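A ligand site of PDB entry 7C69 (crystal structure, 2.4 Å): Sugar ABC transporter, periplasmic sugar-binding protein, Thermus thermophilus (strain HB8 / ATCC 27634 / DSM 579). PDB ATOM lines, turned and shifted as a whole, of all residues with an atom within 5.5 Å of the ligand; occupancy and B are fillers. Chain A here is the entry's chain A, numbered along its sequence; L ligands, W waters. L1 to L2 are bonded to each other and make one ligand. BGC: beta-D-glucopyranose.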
ATOM      1  N   TRP A  42      13.144   5.031 -24.786  1.00  0.00           N
ATOM      2  CA  TRP A  42      14.287   5.923 -25.127  1.00  0.00           C
ATOM      3  C   TRP A  42      14.442   6.094 -26.643  1.00  0.00           C
ATOM      4  O   TRP A  42      14.628   7.200 -27.048  1.00  0.00           O
ATOM      5  CB  TRP A  42      15.589   5.437 -24.490  1.00  0.00           C
ATOM      6  CG  TRP A  42      15.724   5.859 -23.059  1.00  0.00           C
ATOM      7  CD1 TRP A  42      15.700   5.069 -21.947  1.00  0.00           C
ATOM      8  CD2 TRP A  42      15.918   7.206 -22.597  1.00  0.00           C
ATOM      9  NE1 TRP A  42      15.941   5.819 -20.829  1.00  0.00           N
ATOM     10  CE2 TRP A  42      16.046   7.137 -21.192  1.00  0.00           C
ATOM     11  CE3 TRP A  42      16.074   8.438 -23.232  1.00  0.00           C
ATOM     12  CZ2 TRP A  42      16.276   8.272 -20.410  1.00  0.00           C
ATOM     13  CZ3 TRP A  42      16.321   9.549 -22.461  1.00  0.00           C
ATOM     14  CH2 TRP A  42      16.409   9.473 -21.071  1.00  0.00           C
ATOM     15  N   GLY A  65      16.243  13.644 -20.968  1.00  0.00           N
ATOM     16  CA  GLY A  65      17.690  13.447 -20.825  1.00  0.00           C
ATOM     17  C   GLY A  65      18.367  14.790 -20.621  1.00  0.00           C
ATOM     18  O   GLY A  65      17.915  15.718 -21.238  1.00  0.00           O
ATOM     19  N   THR A  66      19.304  14.850 -19.694  1.00  0.00           N
ATOM     20  CA  THR A  66      20.166  16.040 -19.431  1.00  0.00           C
ATOM     21  C   THR A  66      20.700  16.644 -20.733  1.00  0.00           C
ATOM     22  O   THR A  66      20.735  17.834 -20.804  1.00  0.00           O
ATOM     23  CB  THR A  66      21.315  15.715 -18.473  1.00  0.00           C
ATOM     24  OG1 THR A  66      21.963  14.582 -19.038  1.00  0.00           O
ATOM     25  CG2 THR A  66      20.853  15.395 -17.065  1.00  0.00           C
ATOM     26  N   THR A  67      21.122  15.864 -21.719  1.00  0.00           N
ATOM     27  CA  THR A  67      21.740  16.348 -22.998  1.00  0.00           C
ATOM     28  C   THR A  67      20.711  17.004 -23.936  1.00  0.00           C
ATOM     29  O   THR A  67      21.182  17.676 -24.905  1.00  0.00           O
ATOM     30  CB  THR A  67      22.463  15.194 -23.727  1.00  0.00           C
ATOM     31  OG1 THR A  67      21.529  14.388 -24.431  1.00  0.00           O
ATOM     32  CG2 THR A  67      23.263  14.314 -22.774  1.00  0.00           C
ATOM     33  N   TRP A  68      19.400  16.855 -23.667  1.00  0.00           N
ATOM     34  CA  TRP A  68      18.270  17.353 -24.481  1.00  0.00           C
ATOM     35  C   TRP A  68      17.708  18.693 -23.949  1.00  0.00           C
ATOM     36  O   TRP A  68      16.946  19.373 -24.671  1.00  0.00           O
ATOM     37  CB  TRP A  68      17.161  16.291 -24.525  1.00  0.00           C
ATOM     38  CG  TRP A  68      17.537  15.072 -25.321  1.00  0.00           C
ATOM     39  CD1 TRP A  68      18.693  14.889 -26.020  1.00  0.00           C
ATOM     40  CD2 TRP A  68      16.744  13.889 -25.528  1.00  0.00           C
ATOM     41  NE1 TRP A  68      18.662  13.662 -26.632  1.00  0.00           N
ATOM     42  CE2 TRP A  68      17.492  13.038 -26.361  1.00  0.00           C
ATOM     43  CE3 TRP A  68      15.501  13.444 -25.077  1.00  0.00           C
ATOM     44  CZ2 TRP A  68      17.026  11.813 -26.818  1.00  0.00           C
ATOM     45  CZ3 TRP A  68      15.040  12.208 -25.481  1.00  0.00           C
ATOM     46  CH2 TRP A  68      15.801  11.396 -26.328  1.00  0.00           C
ATOM     47  N   GLU A 118      23.363   9.551 -13.535  1.00  0.00           N
ATOM     48  CA  GLU A 118      23.666   8.273 -14.188  1.00  0.00           C
ATOM     49  C   GLU A 118      25.086   8.516 -14.694  1.00  0.00           C
ATOM     50  O   GLU A 118      25.358   9.653 -15.241  1.00  0.00           O
ATOM     51  CB  GLU A 118      22.542   8.151 -15.217  1.00  0.00           C
ATOM     52  CG  GLU A 118      22.492   6.894 -16.026  1.00  0.00           C
ATOM     53  CD  GLU A 118      23.124   7.018 -17.395  1.00  0.00           C
ATOM     54  OE1 GLU A 118      22.461   7.443 -18.387  1.00  0.00           O
ATOM     55  OE2 GLU A 118      24.292   6.672 -17.453  1.00  0.00           O
ATOM     56  N   ARG A 120      28.736   6.051 -16.245  1.00  0.00           N
ATOM     57  CA  ARG A 120      28.991   4.772 -16.952  1.00  0.00           C
ATOM     58  C   ARG A 120      30.220   4.164 -16.302  1.00  0.00           C
ATOM     59  O   ARG A 120      31.113   4.895 -15.856  1.00  0.00           O
ATOM     60  CB  ARG A 120      29.027   4.954 -18.484  1.00  0.00           C
ATOM     61  CG  ARG A 120      27.747   5.548 -19.053  1.00  0.00           C
ATOM     62  CD  ARG A 120      26.498   4.726 -18.775  1.00  0.00           C
ATOM     63  NE  ARG A 120      25.291   5.380 -19.284  1.00  0.00           N
ATOM     64  CZ  ARG A 120      24.930   5.460 -20.546  1.00  0.00           C
ATOM     65  NH1 ARG A 120      25.704   4.957 -21.491  1.00  0.00           N
ATOM     66  NH2 ARG A 120      23.828   6.093 -20.898  1.00  0.00           N
ATOM     67  N   SER A 177      20.483   3.034 -30.412  1.00  0.00           N
ATOM     68  CA  SER A 177      20.554   3.662 -29.062  1.00  0.00           C
ATOM     69  C   SER A 177      21.385   4.939 -28.965  1.00  0.00           C
ATOM     70  O   SER A 177      22.364   5.039 -29.635  1.00  0.00           O
ATOM     71  CB  SER A 177      21.050   2.643 -28.127  1.00  0.00           C
ATOM     72  OG  SER A 177      20.110   1.605 -28.063  1.00  0.00           O
ATOM     73  N   TRP A 178      20.999   5.854 -28.084  1.00  0.00           N
ATOM     74  CA  TRP A 178      21.762   7.091 -27.789  1.00  0.00           C
ATOM     75  C   TRP A 178      23.127   6.708 -27.229  1.00  0.00           C
ATOM     76  O   TRP A 178      24.037   7.475 -27.397  1.00  0.00           O
ATOM     77  CB  TRP A 178      21.009   8.043 -26.852  1.00  0.00           C
ATOM     78  CG  TRP A 178      19.591   8.264 -27.266  1.00  0.00           C
ATOM     79  CD1 TRP A 178      18.475   7.800 -26.634  1.00  0.00           C
ATOM     80  CD2 TRP A 178      19.114   8.960 -28.425  1.00  0.00           C
ATOM     81  NE1 TRP A 178      17.366   8.154 -27.327  1.00  0.00           N
ATOM     82  CE2 TRP A 178      17.717   8.847 -28.435  1.00  0.00           C
ATOM     83  CE3 TRP A 178      19.734   9.616 -29.495  1.00  0.00           C
ATOM     84  CZ2 TRP A 178      16.921   9.425 -29.422  1.00  0.00           C
ATOM     85  CZ3 TRP A 178      18.956  10.178 -30.481  1.00  0.00           C
ATOM     86  CH2 TRP A 178      17.567  10.067 -30.450  1.00  0.00           C
ATOM     87  N   ASP A 179      23.244   5.497 -26.697  1.00  0.00           N
ATOM     88  CA  ASP A 179      24.537   5.024 -26.121  1.00  0.00           C
ATOM     89  C   ASP A 179      25.586   4.771 -27.213  1.00  0.00           C
ATOM     90  O   ASP A 179      26.770   4.646 -26.861  1.00  0.00           O
ATOM     91  CB  ASP A 179      24.369   3.767 -25.279  1.00  0.00           C
ATOM     92  CG  ASP A 179      23.581   3.942 -24.001  1.00  0.00           C
ATOM     93  OD1 ASP A 179      23.590   5.025 -23.439  1.00  0.00           O
ATOM     94  OD2 ASP A 179      22.908   2.995 -23.613  1.00  0.00           O
ATOM     95  N   HIS A 182      27.207   7.743 -26.403  1.00  0.00           N
ATOM     96  CA  HIS A 182      27.669   7.839 -24.993  1.00  0.00           C
ATOM     97  C   HIS A 182      28.753   6.803 -24.687  1.00  0.00           C
ATOM     98  O   HIS A 182      29.594   7.090 -23.788  1.00  0.00           O
ATOM     99  CB  HIS A 182      26.489   7.807 -24.034  1.00  0.00           C
ATOM    100  CG  HIS A 182      25.327   8.658 -24.421  1.00  0.00           C
ATOM    101  ND1 HIS A 182      25.454   9.965 -24.797  1.00  0.00           N
ATOM    102  CD2 HIS A 182      24.000   8.389 -24.371  1.00  0.00           C
ATOM    103  CE1 HIS A 182      24.262  10.464 -24.982  1.00  0.00           C
ATOM    104  NE2 HIS A 182      23.334   9.527 -24.676  1.00  0.00           N
ATOM    105  N   THR A 237      21.032  -1.026 -27.056  1.00  0.00           N
ATOM    106  CA  THR A 237      21.453  -1.098 -25.632  1.00  0.00           C
ATOM    107  C   THR A 237      20.697  -2.227 -24.927  1.00  0.00           C
ATOM    108  O   THR A 237      21.334  -3.027 -24.177  1.00  0.00           O
ATOM    109  CB  THR A 237      21.281   0.257 -24.959  1.00  0.00           C
ATOM    110  OG1 THR A 237      22.285   1.117 -25.503  1.00  0.00           O
ATOM    111  CG2 THR A 237      21.388   0.196 -23.442  1.00  0.00           C
ATOM    112  N   ALA A 238      19.378  -2.276 -25.094  1.00  0.00           N
ATOM    113  CA  ALA A 238      18.515  -3.177 -24.311  1.00  0.00           C
ATOM    114  C   ALA A 238      18.959  -4.615 -24.601  1.00  0.00           C
ATOM    115  O   ALA A 238      19.018  -5.441 -23.671  1.00  0.00           O
ATOM    116  CB  ALA A 238      17.071  -2.923 -24.675  1.00  0.00           C
ATOM    117  N   GLU A 241      22.324  -5.346 -22.844  1.00  0.00           N
ATOM    118  CA  GLU A 241      21.925  -5.544 -21.420  1.00  0.00           C
ATOM    119  C   GLU A 241      21.430  -6.979 -21.265  1.00  0.00           C
ATOM    120  O   GLU A 241      21.926  -7.667 -20.363  1.00  0.00           O
ATOM    121  CB  GLU A 241      20.823  -4.562 -21.002  1.00  0.00           C
ATOM    122  CG  GLU A 241      21.350  -3.210 -20.630  1.00  0.00           C
ATOM    123  CD  GLU A 241      20.284  -2.127 -20.477  1.00  0.00           C
ATOM    124  OE1 GLU A 241      19.085  -2.418 -20.652  1.00  0.00           O
ATOM    125  OE2 GLU A 241      20.684  -0.992 -20.165  1.00  0.00           O
ATOM    126  N   TRP A 257      22.017   1.372 -12.484  1.00  0.00           N
ATOM    127  CA  TRP A 257      20.719   0.661 -12.439  1.00  0.00           C
ATOM    128  C   TRP A 257      20.899  -0.856 -12.479  1.00  0.00           C
ATOM    129  O   TRP A 257      20.057  -1.559 -11.855  1.00  0.00           O
ATOM    130  CB  TRP A 257      19.798   1.161 -13.563  1.00  0.00           C
ATOM    131  CG  TRP A 257      20.298   0.906 -14.950  1.00  0.00           C
ATOM    132  CD1 TRP A 257      20.143  -0.240 -15.681  1.00  0.00           C
ATOM    133  CD2 TRP A 257      20.947   1.853 -15.822  1.00  0.00           C
ATOM    134  NE1 TRP A 257      20.710  -0.072 -16.923  1.00  0.00           N
ATOM    135  CE2 TRP A 257      21.222   1.183 -17.027  1.00  0.00           C
ATOM    136  CE3 TRP A 257      21.312   3.191 -15.708  1.00  0.00           C
ATOM    137  CZ2 TRP A 257      21.817   1.816 -18.119  1.00  0.00           C
ATOM    138  CZ3 TRP A 257      21.963   3.819 -16.762  1.00  0.00           C
ATOM    139  CH2 TRP A 257      22.190   3.138 -17.977  1.00  0.00           C
ATOM    140  N   PHE A 295      31.177   9.080 -19.150  1.00  0.00           N
ATOM    141  CA  PHE A 295      29.973   9.845 -19.503  1.00  0.00           C
ATOM    142  C   PHE A 295      29.163  10.045 -18.223  1.00  0.00           C
ATOM    143  O   PHE A 295      28.832   9.060 -17.539  1.00  0.00           O
ATOM    144  CB  PHE A 295      29.168   9.117 -20.569  1.00  0.00           C
ATOM    145  CG  PHE A 295      27.791   9.713 -20.761  1.00  0.00           C
ATOM    146  CD1 PHE A 295      27.651  10.866 -21.469  1.00  0.00           C
ATOM    147  CD2 PHE A 295      26.684   9.172 -20.153  1.00  0.00           C
ATOM    148  CE1 PHE A 295      26.405  11.426 -21.664  1.00  0.00           C
ATOM    149  CE2 PHE A 295      25.451   9.773 -20.283  1.00  0.00           C
ATOM    150  CZ  PHE A 295      25.303  10.884 -21.047  1.00  0.00           C
ATOM    151  N   PHE A 296      28.845  11.304 -17.926  1.00  0.00           N
ATOM    152  CA  PHE A 296      27.930  11.706 -16.841  1.00  0.00           C
ATOM    153  C   PHE A 296      26.713  12.317 -17.486  1.00  0.00           C
ATOM    154  O   PHE A 296      26.837  13.212 -18.265  1.00  0.00           O
ATOM    155  CB  PHE A 296      28.651  12.661 -15.877  1.00  0.00           C
ATOM    156  CG  PHE A 296      27.893  12.909 -14.596  1.00  0.00           C
ATOM    157  CD1 PHE A 296      26.787  13.727 -14.587  1.00  0.00           C
ATOM    158  CD2 PHE A 296      28.265  12.311 -13.395  1.00  0.00           C
ATOM    159  CE1 PHE A 296      26.087  13.967 -13.415  1.00  0.00           C
ATOM    160  CE2 PHE A 296      27.573  12.572 -12.213  1.00  0.00           C
ATOM    161  CZ  PHE A 296      26.480  13.399 -12.221  1.00  0.00           C
ATOM    162  N   GLY A 297      25.555  11.719 -17.218  1.00  0.00           N
ATOM    163  CA  GLY A 297      24.238  12.152 -17.707  1.00  0.00           C
ATOM    164  C   GLY A 297      23.187  11.896 -16.645  1.00  0.00           C
ATOM    165  O   GLY A 297      23.471  12.109 -15.437  1.00  0.00           O
ATOM    166  N   GLY A 298      22.042  11.410 -17.083  1.00  0.00           N
ATOM    167  CA  GLY A 298      20.827  11.345 -16.279  1.00  0.00           C
ATOM    168  C   GLY A 298      19.659  12.054 -16.960  1.00  0.00           C
ATOM    169  O   GLY A 298      19.682  12.280 -18.177  1.00  0.00           O
ATOM    170  N   SER A 299      18.617  12.314 -16.176  1.00  0.00           N
ATOM    171  CA  SER A 299      17.353  12.871 -16.667  1.00  0.00           C
ATOM    172  C   SER A 299      16.937  13.994 -15.714  1.00  0.00           C
ATOM    173  O   SER A 299      17.209  13.918 -14.485  1.00  0.00           O
ATOM    174  CB  SER A 299      16.306  11.806 -16.833  1.00  0.00           C
ATOM    175  OG  SER A 299      16.544  10.980 -17.979  1.00  0.00           O
ATOM    176  N   MET A 335      19.449   4.407  -9.767  1.00  0.00           N
ATOM    177  CA  MET A 335      20.149   5.602 -10.255  1.00  0.00           C
ATOM    178  C   MET A 335      20.787   6.287  -9.053  1.00  0.00           C
ATOM    179  O   MET A 335      20.539   5.801  -7.918  1.00  0.00           O
ATOM    180  CB  MET A 335      19.196   6.555 -10.964  1.00  0.00           C
ATOM    181  CG  MET A 335      18.552   5.908 -12.194  1.00  0.00           C
ATOM    182  SD  MET A 335      19.660   5.527 -13.555  1.00  0.00           S
ATOM    183  CE  MET A 335      18.427   5.321 -14.843  1.00  0.00           C
ATOM    184  N   GLU A 377      22.864  14.295 -31.662  1.00  0.00           N
ATOM    185  CA  GLU A 377      22.823  12.900 -31.181  1.00  0.00           C
ATOM    186  C   GLU A 377      22.278  12.010 -32.318  1.00  0.00           C
ATOM    187  O   GLU A 377      22.906  10.987 -32.624  1.00  0.00           O
ATOM    188  CB  GLU A 377      22.090  12.840 -29.844  1.00  0.00           C
ATOM    189  CG  GLU A 377      22.872  13.454 -28.700  1.00  0.00           C
ATOM    190  CD  GLU A 377      22.371  13.064 -27.314  1.00  0.00           C
ATOM    191  OE1 GLU A 377      21.280  12.442 -27.252  1.00  0.00           O
ATOM    192  OE2 GLU A 377      23.082  13.313 -26.296  1.00  0.00           O
HETATM  193  C2  BGC L   1      20.098   6.483 -21.592  1.00  0.00           C
HETATM  194  C3  BGC L   1      20.410   5.288 -20.729  1.00  0.00           C
HETATM  195  C4  BGC L   1      19.518   4.113 -21.042  1.00  0.00           C
HETATM  196  C5  BGC L   1      19.517   3.834 -22.538  1.00  0.00           C
HETATM  197  C6  BGC L   1      18.610   2.723 -23.029  1.00  0.00           C
HETATM  198  C1  BGC L   1      20.112   6.015 -23.048  1.00  0.00           C
HETATM  199  O1  BGC L   1      19.848   7.040 -23.987  1.00  0.00           O
HETATM  200  O2  BGC L   1      21.038   7.506 -21.263  1.00  0.00           O
HETATM  201  O3  BGC L   1      20.217   5.734 -19.399  1.00  0.00           O
HETATM  202  O4  BGC L   1      19.912   2.956 -20.273  1.00  0.00           O
HETATM  203  O5  BGC L   1      19.078   5.033 -23.189  1.00  0.00           O
HETATM  204  O6  BGC L   1      18.489   2.917 -24.457  1.00  0.00           O
HETATM  205  C2  BGC L   2      21.369   9.763 -20.547  1.00  0.00           C
HETATM  206  C3  BGC L   2      21.043  11.221 -20.823  1.00  0.00           C
HETATM  207  C4  BGC L   2      20.966  11.529 -22.307  1.00  0.00           C
HETATM  208  C5  BGC L   2      20.022  10.524 -22.959  1.00  0.00           C
HETATM  209  C6  BGC L   2      19.798  10.811 -24.449  1.00  0.00           C
HETATM  210  C1  BGC L   2      20.520   8.811 -21.378  1.00  0.00           C
HETATM  211  O2  BGC L   2      21.160   9.523 -19.158  1.00  0.00           O
HETATM  212  O3  BGC L   2      22.041  12.033 -20.151  1.00  0.00           O
HETATM  213  O4  BGC L   2      20.508  12.891 -22.446  1.00  0.00           O
HETATM  214  O5  BGC L   2      20.519   9.182 -22.770  1.00  0.00           O
HETATM  215  O6  BGC L   2      21.042  10.943 -25.182  1.00  0.00           O
HETATM  216  O   HOH W   1      18.028   4.305 -26.938  1.00  0.00           O
HETATM  217  O   HOH W   2      17.328   0.208 -25.463  1.00  0.00           O
HETATM  218  O   HOH W   3      18.660   9.383 -17.887  1.00  0.00           O
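Residues that only touch the ligand: Trp 42, Gly 65, Trp 68, Trp 178, Asp 179, Thr 237, Trp 257, Phe 295 and Gly 297.
The side-chain carboxylate (OE2) of Glu 377 lies within hydrogen-bond range of the side-chain hydroxyl (OG1) of Thr 67.
The backbone carbonyl oxygen (O) of Trp 178 sits close to a ring nitrogen (NE2) of His 182 (3.5 Å).
The backbone carbonyl oxygen of Gly 298 is in hydrogen-bond range of the backbone NH of Thr 66, at 3.0 Å.
The backbone carbonyl oxygen (O) of Trp 42 is in hydrogen-bond range of the indole nitrogen (NE1) of Trp 178, at 2.9 Å.
The backbone carbonyl oxygen of Phe 295 lies within hydrogen-bond range of the backbone NH of Arg 120, 3.3 Å away.
The guanidinium group (NH2) of Arg 120 is in salt-bridge range of the side-chain carboxylate (OD1) of Asp 179 (2.8 Å).
OD2 of Asp 179 lies within hydrogen-bond range of OG1 of Thr 237, 2.7 Å away.
The side-chain hydroxyl of Ser 177 is in hydrogen-bond range of the backbone NH of Thr 237 (3.0 Å).
Water W3 lies within hydrogen-bond range of OG of Ser 299, O2 of BGC L2 and O of Gly 298.
Water W2 lies within hydrogen-bond range of O6 of BGC L1 (3.1 Å) and N of Ala 238 (3.2 Å).
The side-chain carboxylate (OE1) of Glu 377 is in hydrogen-bond range of an oxygen (O6) of BGC L2, 2.6 Å away.
OE1 of Glu 118 is in hydrogen-bond range of O2 of BGC L2, at 2.6 Å.
The backbone NH of Thr 67 sits close to an oxygen (O4) of BGC L2, at 3.1 Å.
OG1 of Thr 67 lies within hydrogen-bond range of O4 of BGC L2, 2.7 Å away.
An oxygen (O6) of BGC L2 sits at hydrogen-bond distance from a ring nitrogen (NE2) of His 182 (2.7 Å).
An oxygen (O3) of BGC L2 lies within hydrogen-bond range of the side-chain hydroxyl of Thr 66 (2.8 Å).
An oxygen (O2) of BGC L2 sits at hydrogen-bond distance from the backbone NH (N) of Gly 298, at 2.9 Å.
The backbone carbonyl oxygen of Gly 298 lies within hydrogen-bond range of an oxygen (O3) of BGC L2, at 3.1 Å.
The guanidinium group of Arg 120 is in hydrogen-bond range of an oxygen (O2) of BGC L1, at 3.1 Å.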
